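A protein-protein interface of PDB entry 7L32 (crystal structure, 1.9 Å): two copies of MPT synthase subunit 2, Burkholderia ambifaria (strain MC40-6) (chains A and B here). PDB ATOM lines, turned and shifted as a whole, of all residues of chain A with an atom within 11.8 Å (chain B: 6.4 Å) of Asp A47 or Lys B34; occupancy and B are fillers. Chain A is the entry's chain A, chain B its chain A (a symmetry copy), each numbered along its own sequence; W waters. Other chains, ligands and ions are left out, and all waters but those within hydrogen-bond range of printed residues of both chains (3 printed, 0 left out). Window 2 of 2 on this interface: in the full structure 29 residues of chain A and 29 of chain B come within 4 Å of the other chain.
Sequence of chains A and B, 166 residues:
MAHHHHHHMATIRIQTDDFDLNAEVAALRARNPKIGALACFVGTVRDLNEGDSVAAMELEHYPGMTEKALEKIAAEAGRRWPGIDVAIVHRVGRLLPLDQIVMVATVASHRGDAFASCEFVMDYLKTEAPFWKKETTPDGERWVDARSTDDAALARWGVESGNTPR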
ATOM      1  N   VAL A  42     -11.100  19.287 -14.380  1.00  0.00           N
ATOM      2  CA  VAL A  42     -11.027  20.737 -14.524  1.00  0.00           C
ATOM      3  C   VAL A  42     -12.126  21.360 -13.679  1.00  0.00           C
ATOM      4  O   VAL A  42     -13.311  21.074 -13.885  1.00  0.00           O
ATOM      5  CB  VAL A  42     -11.168  21.193 -15.987  1.00  0.00           C
ATOM      6  CG1 VAL A  42     -11.139  22.722 -16.067  1.00  0.00           C
ATOM      7  CG2 VAL A  42     -10.042  20.600 -16.837  1.00  0.00           C
ATOM      8  N   GLY A  43     -11.743  22.245 -12.761  1.00  0.00           N
ATOM      9  CA  GLY A  43     -12.700  23.014 -11.986  1.00  0.00           C
ATOM     10  C   GLY A  43     -12.798  24.430 -12.524  1.00  0.00           C
ATOM     11  O   GLY A  43     -11.793  25.020 -12.920  1.00  0.00           O
ATOM     12  N   THR A  44     -14.020  24.969 -12.537  1.00  0.00           N
ATOM     13  CA  THR A  44     -14.327  26.284 -13.100  1.00  0.00           C
ATOM     14  C   THR A  44     -15.203  27.065 -12.140  1.00  0.00           C
ATOM     15  O   THR A  44     -16.037  26.480 -11.440  1.00  0.00           O
ATOM     16  CB  THR A  44     -15.071  26.199 -14.456  1.00  0.00           C
ATOM     17  OG1 THR A  44     -16.225  25.357 -14.324  1.00  0.00           O
ATOM     18  CG2 THR A  44     -14.163  25.645 -15.557  1.00  0.00           C
ATOM     19  N   VAL A  45     -15.023  28.397 -12.135  1.00  0.00           N
ATOM     20  CA  VAL A  45     -15.809  29.273 -11.268  1.00  0.00           C
ATOM     21  C   VAL A  45     -17.291  29.069 -11.549  1.00  0.00           C
ATOM     22  O   VAL A  45     -17.772  29.323 -12.661  1.00  0.00           O
ATOM     23  CB  VAL A  45     -15.418  30.748 -11.471  1.00  0.00           C
ATOM     24  CG1 VAL A  45     -16.257  31.646 -10.560  1.00  0.00           C
ATOM     25  CG2 VAL A  45     -13.921  30.958 -11.227  1.00  0.00           C
ATOM     26  N   ARG A  46     -18.026  28.619 -10.535  1.00  0.00           N
ATOM     27  CA  ARG A  46     -19.439  28.334 -10.725  1.00  0.00           C
ATOM     28  C   ARG A  46     -20.224  29.635 -10.878  1.00  0.00           C
ATOM     29  O   ARG A  46     -19.951  30.632 -10.203  1.00  0.00           O
ATOM     30  CB  ARG A  46     -19.966  27.493  -9.563  1.00  0.00           C
ATOM     31  CG  ARG A  46     -21.125  26.573  -9.939  1.00  0.00           C
ATOM     32  CD  ARG A  46     -21.672  25.850  -8.715  1.00  0.00           C
ATOM     33  NE  ARG A  46     -22.889  25.099  -9.007  1.00  0.00           N
ATOM     34  CZ  ARG A  46     -23.682  24.582  -8.077  1.00  0.00           C
ATOM     35  NH1 ARG A  46     -23.398  24.695  -6.788  1.00  0.00           N
ATOM     36  NH2 ARG A  46     -24.804  23.965  -8.446  1.00  0.00           N
ATOM     37  N   ASP A  47     -21.211  29.620 -11.774  1.00  0.00           N
ATOM     38  CA  ASP A  47     -22.008  30.812 -12.075  1.00  0.00           C
ATOM     39  C   ASP A  47     -23.225  30.824 -11.150  1.00  0.00           C
ATOM     40  O   ASP A  47     -24.350  30.501 -11.537  1.00  0.00           O
ATOM     41  CB  ASP A  47     -22.395  30.808 -13.551  1.00  0.00           C
ATOM     42  CG  ASP A  47     -23.010  32.116 -14.018  1.00  0.00           C
ATOM     43  OD1 ASP A  47     -22.894  33.151 -13.319  1.00  0.00           O
ATOM     44  OD2 ASP A  47     -23.617  32.098 -15.109  1.00  0.00           O
ATOM     45  N   LEU A  48     -22.987  31.238  -9.906  1.00  0.00           N
ATOM     46  CA  LEU A  48     -24.026  31.260  -8.875  1.00  0.00           C
ATOM     47  C   LEU A  48     -24.585  32.665  -8.659  1.00  0.00           C
ATOM     48  O   LEU A  48     -23.939  33.507  -8.034  1.00  0.00           O
ATOM     49  CB  LEU A  48     -23.478  30.714  -7.553  1.00  0.00           C
ATOM     50  N   ALA A  56     -16.732  38.722  -8.348  1.00  0.00           N
ATOM     51  CA  ALA A  56     -15.607  37.976  -8.899  1.00  0.00           C
ATOM     52  C   ALA A  56     -14.777  37.342  -7.792  1.00  0.00           C
ATOM     53  O   ALA A  56     -14.683  37.872  -6.683  1.00  0.00           O
ATOM     54  CB  ALA A  56     -14.735  38.881  -9.755  1.00  0.00           C
ATOM     55  N   MET A  57     -14.156  36.213  -8.113  1.00  0.00           N
ATOM     56  CA  MET A  57     -13.282  35.510  -7.183  1.00  0.00           C
ATOM     57  C   MET A  57     -11.853  35.997  -7.379  1.00  0.00           C
ATOM     58  O   MET A  57     -11.315  35.928  -8.488  1.00  0.00           O
ATOM     59  CB  MET A  57     -13.384  33.997  -7.399  1.00  0.00           C
ATOM     60  CG  MET A  57     -12.427  33.155  -6.540  1.00  0.00           C
ATOM     61  SD  MET A  57     -12.358  31.395  -6.957  1.00  0.00           S
ATOM     62  CE  MET A  57     -13.979  31.109  -7.674  1.00  0.00           C
ATOM     63  N   LEU A  95     -10.681  35.936 -11.076  1.00  0.00           N
ATOM     64  CA  LEU A  95     -11.301  34.911 -11.910  1.00  0.00           C
ATOM     65  C   LEU A  95     -12.803  35.145 -11.956  1.00  0.00           C
ATOM     66  O   LEU A  95     -13.438  35.327 -10.912  1.00  0.00           O
ATOM     67  CB  LEU A  95     -10.995  33.515 -11.374  1.00  0.00           C
ATOM     68  CG  LEU A  95      -9.507  33.176 -11.224  1.00  0.00           C
ATOM     69  CD1 LEU A  95      -9.330  31.944 -10.343  1.00  0.00           C
ATOM     70  CD2 LEU A  95      -8.842  32.962 -12.586  1.00  0.00           C
ATOM     71  N   LEU A  96     -13.363  35.159 -13.167  1.00  0.00           N
ATOM     72  CA  LEU A  96     -14.778  35.430 -13.388  1.00  0.00           C
ATOM     73  C   LEU A  96     -15.574  34.131 -13.438  1.00  0.00           C
ATOM     74  O   LEU A  96     -15.005  33.052 -13.625  1.00  0.00           O
ATOM     75  CB  LEU A  96     -14.964  36.212 -14.691  1.00  0.00           C
ATOM     76  CG  LEU A  96     -14.427  37.645 -14.640  1.00  0.00           C
ATOM     77  CD1 LEU A  96     -14.572  38.349 -15.988  1.00  0.00           C
ATOM     78  CD2 LEU A  96     -15.145  38.422 -13.551  1.00  0.00           C
ATOM     79  N   PRO A  97     -16.897  34.205 -13.279  1.00  0.00           N
ATOM     80  CA  PRO A  97     -17.731  33.019 -13.504  1.00  0.00           C
ATOM     81  C   PRO A  97     -17.457  32.407 -14.868  1.00  0.00           C
ATOM     82  O   PRO A  97     -17.320  33.111 -15.874  1.00  0.00           O
ATOM     83  CB  PRO A  97     -19.162  33.565 -13.409  1.00  0.00           C
ATOM     84  CG  PRO A  97     -19.035  34.780 -12.528  1.00  0.00           C
ATOM     85  CD  PRO A  97     -17.694  35.371 -12.850  1.00  0.00           C
ATOM     86  N   LEU A  98     -17.376  31.081 -14.884  1.00  0.00           N
ATOM     87  CA  LEU A  98     -17.107  30.201 -16.016  1.00  0.00           C
ATOM     88  C   LEU A  98     -15.608  30.071 -16.301  1.00  0.00           C
ATOM     89  O   LEU A  98     -15.226  29.201 -17.084  1.00  0.00           O
ATOM     90  CB  LEU A  98     -17.842  30.617 -17.308  1.00  0.00           C
ATOM     91  CG  LEU A  98     -19.359  30.772 -17.175  1.00  0.00           C
ATOM     92  CD1 LEU A  98     -19.994  31.213 -18.497  1.00  0.00           C
ATOM     93  CD2 LEU A  98     -19.999  29.500 -16.647  1.00  0.00           C
ATOM     94  N   ASP A  99     -14.745  30.881 -15.679  1.00  0.00           N
ATOM     95  CA  ASP A  99     -13.309  30.740 -15.880  1.00  0.00           C
ATOM     96  C   ASP A  99     -12.814  29.410 -15.324  1.00  0.00           C
ATOM     97  O   ASP A  99     -13.252  28.966 -14.260  1.00  0.00           O
ATOM     98  CB  ASP A  99     -12.544  31.857 -15.163  1.00  0.00           C
ATOM     99  CG  ASP A  99     -12.591  33.184 -15.895  1.00  0.00           C
ATOM    100  OD1 ASP A  99     -13.081  33.260 -17.042  1.00  0.00           O
ATOM    101  OD2 ASP A  99     -12.151  34.169 -15.281  1.00  0.00           O
ATOM    102  N   GLN A 100     -11.850  28.812 -16.016  1.00  0.00           N
ATOM    103  CA  GLN A 100     -11.126  27.674 -15.459  1.00  0.00           C
ATOM    104  C   GLN A 100     -10.310  28.106 -14.249  1.00  0.00           C
ATOM    105  O   GLN A 100      -9.661  29.158 -14.268  1.00  0.00           O
ATOM    106  CB  GLN A 100     -10.198  27.069 -16.508  1.00  0.00           C
ATOM    107  CG  GLN A 100     -10.921  26.459 -17.701  1.00  0.00           C
ATOM    108  CD  GLN A 100      -9.977  25.841 -18.726  1.00  0.00           C
ATOM    109  OE1 GLN A 100     -10.199  24.721 -19.183  1.00  0.00           O
ATOM    110  NE2 GLN A 100      -8.938  26.584 -19.116  1.00  0.00           N
ATOM    111  N   ILE A 101     -10.329  27.280 -13.204  1.00  0.00           N
ATOM    112  CA  ILE A 101      -9.536  27.512 -11.983  1.00  0.00           C
ATOM    113  C   ILE A 101      -8.335  26.583 -11.917  1.00  0.00           C
ATOM    114  O   ILE A 101      -7.214  27.006 -11.645  1.00  0.00           O
ATOM    115  CB  ILE A 101     -10.411  27.322 -10.722  1.00  0.00           C
ATOM    116  CG1 ILE A 101     -11.600  28.270 -10.709  1.00  0.00           C
ATOM    117  CG2 ILE A 101      -9.585  27.508  -9.447  1.00  0.00           C
ATOM    118  CD1 ILE A 101     -12.632  27.866  -9.668  1.00  0.00           C
ATOM    119  N   ARG B  29     -19.774  21.755 -21.394  1.00  0.00           N
ATOM    120  CA  ARG B  29     -19.984  22.887 -20.495  1.00  0.00           C
ATOM    121  C   ARG B  29     -21.065  23.818 -21.024  1.00  0.00           C
ATOM    122  O   ARG B  29     -21.868  24.361 -20.253  1.00  0.00           O
ATOM    123  CB  ARG B  29     -18.678  23.666 -20.304  1.00  0.00           C
ATOM    124  CG  ARG B  29     -17.558  22.897 -19.644  1.00  0.00           C
ATOM    125  CD  ARG B  29     -16.448  23.872 -19.225  1.00  0.00           C
ATOM    126  NE  ARG B  29     -15.417  23.249 -18.403  1.00  0.00           N
ATOM    127  CZ  ARG B  29     -15.528  23.022 -17.100  1.00  0.00           C
ATOM    128  NH1 ARG B  29     -16.640  23.298 -16.444  1.00  0.00           N
ATOM    129  NH2 ARG B  29     -14.489  22.519 -16.435  1.00  0.00           N
ATOM    130  N   ASN B  32     -24.429  22.846 -19.996  1.00  0.00           N
ATOM    131  CA  ASN B  32     -24.608  22.766 -18.543  1.00  0.00           C
ATOM    132  C   ASN B  32     -24.124  24.064 -17.903  1.00  0.00           C
ATOM    133  O   ASN B  32     -23.087  24.105 -17.223  1.00  0.00           O
ATOM    134  CB  ASN B  32     -23.893  21.534 -17.984  1.00  0.00           C
ATOM    135  CG  ASN B  32     -24.513  20.252 -18.497  1.00  0.00           C
ATOM    136  OD1 ASN B  32     -25.520  19.794 -17.948  1.00  0.00           O
ATOM    137  ND2 ASN B  32     -23.973  19.708 -19.597  1.00  0.00           N
ATOM    138  N   PRO B  33     -24.870  25.155 -18.094  1.00  0.00           N
ATOM    139  CA  PRO B  33     -24.352  26.488 -17.730  1.00  0.00           C
ATOM    140  C   PRO B  33     -24.165  26.733 -16.230  1.00  0.00           C
ATOM    141  O   PRO B  33     -23.477  27.702 -15.872  1.00  0.00           O
ATOM    142  CB  PRO B  33     -25.397  27.444 -18.325  1.00  0.00           C
ATOM    143  CG  PRO B  33     -26.684  26.617 -18.388  1.00  0.00           C
ATOM    144  CD  PRO B  33     -26.200  25.225 -18.744  1.00  0.00           C
ATOM    145  N   LYS B  34     -24.765  25.932 -15.344  1.00  0.00           N
ATOM    146  CA  LYS B  34     -24.773  26.258 -13.920  1.00  0.00           C
ATOM    147  C   LYS B  34     -23.918  25.322 -13.077  1.00  0.00           C
ATOM    148  O   LYS B  34     -23.890  25.470 -11.853  1.00  0.00           O
ATOM    149  CB  LYS B  34     -26.211  26.274 -13.376  1.00  0.00           C
ATOM    150  CG  LYS B  34     -27.142  27.230 -14.122  1.00  0.00           C
ATOM    151  CD  LYS B  34     -26.667  28.685 -14.042  1.00  0.00           C
ATOM    152  CE  LYS B  34     -27.021  29.303 -12.703  1.00  0.00           C
ATOM    153  NZ  LYS B  34     -26.759  30.755 -12.732  1.00  0.00           N
ATOM    154  N   ILE B  35     -23.221  24.364 -13.677  1.00  0.00           N
ATOM    155  CA  ILE B  35     -22.370  23.477 -12.888  1.00  0.00           C
ATOM    156  C   ILE B  35     -20.991  23.462 -13.521  1.00  0.00           C
ATOM    157  O   ILE B  35     -20.855  23.611 -14.738  1.00  0.00           O
ATOM    158  CB  ILE B  35     -22.957  22.054 -12.749  1.00  0.00           C
ATOM    159  CG1 ILE B  35     -23.304  21.448 -14.124  1.00  0.00           C
ATOM    160  CG2 ILE B  35     -24.201  22.077 -11.845  1.00  0.00           C
ATOM    161  CD1 ILE B  35     -23.919  20.061 -14.010  1.00  0.00           C
ATOM    162  N   GLY B  36     -19.958  23.328 -12.678  1.00  0.00           N
ATOM    163  CA  GLY B  36     -18.591  23.502 -13.141  1.00  0.00           C
ATOM    164  C   GLY B  36     -17.531  22.449 -12.835  1.00  0.00           C
ATOM    165  O   GLY B  36     -16.359  22.698 -13.125  1.00  0.00           O
ATOM    166  N   SER B 109     -22.221  19.461 -10.200  1.00  0.00           N
ATOM    167  CA  SER B 109     -21.992  20.614  -9.345  1.00  0.00           C
ATOM    168  C   SER B 109     -20.735  20.440  -8.494  1.00  0.00           C
ATOM    169  O   SER B 109     -20.093  21.437  -8.134  1.00  0.00           O
ATOM    170  CB  SER B 109     -23.221  20.869  -8.462  1.00  0.00           C
ATOM    171  OG  SER B 109     -23.431  19.801  -7.564  1.00  0.00           O
HETATM  172  O   HOH W   1     -23.998  30.262 -16.988  1.00  0.00           O
HETATM  173  O   HOH W   2     -21.288  27.367 -13.954  1.00  0.00           O
HETATM  174  O   HOH W   3     -18.334  25.715 -16.801  1.00  0.00           O
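O of Gly B36 touches O of Val A42, at 3.5 Å.
O of Gly B36 touches CA of Gly A43 (3.8 Å).
Ile B35 touches Arg A46.
Arg A46 touches Ser B109 (NH2 to CB, 3.5 Å).
Pro B33 touches Leu A98.
No position is printed for both chains.
Asp A47 touches just one residue of chain B: Lys B34 (2.7 Å).
No residue of chain A comes within 4 Å of Asn B32.
Of the printed residues of chain A, Ile B35 touches Arg A46 (3.9 Å).
Of the printed residues of chain B, Gly A43 touches Gly B36.
Printed residues of chain A within 4 Å of Gly B36: Val A42, Gly A43 and Thr A44.
Leu A95 touches none of the printed residues of chain B.
The nearest residue of chain A that does not touch Lys B34 is Leu A48 (4.7 Å).
Water W1 bridges the side-chain carboxylate of Asp A47 (2.7 Å) and the backbone carbonyl oxygen of Pro B33 (2.8 Å).
Water W2 lies within hydrogen-bond range of the backbone carbonyl oxygen of Pro B33 and the backbone NH of Asp A47.
Water W3 lies within hydrogen-bond range of NH1 of Arg B29 and OG1 of Thr A44.
Of the 7 printed residues of chain B, 6 touch a printed residue of chain A.
Hydrophobic or aromatic side chains of chain B that line the printed part of chain A: Ile B35.
Along chain B the printed residues that touch a printed residue of chain A span positions 29 to 109.
Hydrophobic or aromatic side chains of chain A within 4 Å of the printed part of chain B: Val A42 and Leu A98.
Among the printed residues, 10 pairs touch across the chains.
Among the printed residues, no Asp or Glu carboxylate lies within 4 Å of a Lys or Arg side-chain nitrogen of the other chain.
The backbone carbonyl oxygen of Val A42 sits at hydrogen-bond distance from the guanidinium group of Arg B29, at 3.2 Å.
The guanidinium group (NH1) of Arg B29 sits at hydrogen-bond distance from the side-chain hydroxyl (OG1) of Thr A44 (3.0 Å).
OG1 of Thr A44 sits at hydrogen-bond distance from O of Gly B36, at 2.9 Å.
The backbone carbonyl oxygen of Lys B34 is in hydrogen-bond range of the guanidinium group of Arg A46 (3.0 Å).
NZ of Lys B34 lies within hydrogen-bond range of O of Asp A47 (2.7 Å).
The backbone NH (N) of Ile A101 is in hydrogen-bond range of the backbone carbonyl oxygen (O) of Gly A43.
The backbone NH (N) of Leu A98 is in hydrogen-bond range of the backbone carbonyl oxygen (O) of Val A45, 2.9 Å away.
NH1 of Arg B29 sits at hydrogen-bond distance from O of Gly B36 (3.4 Å).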
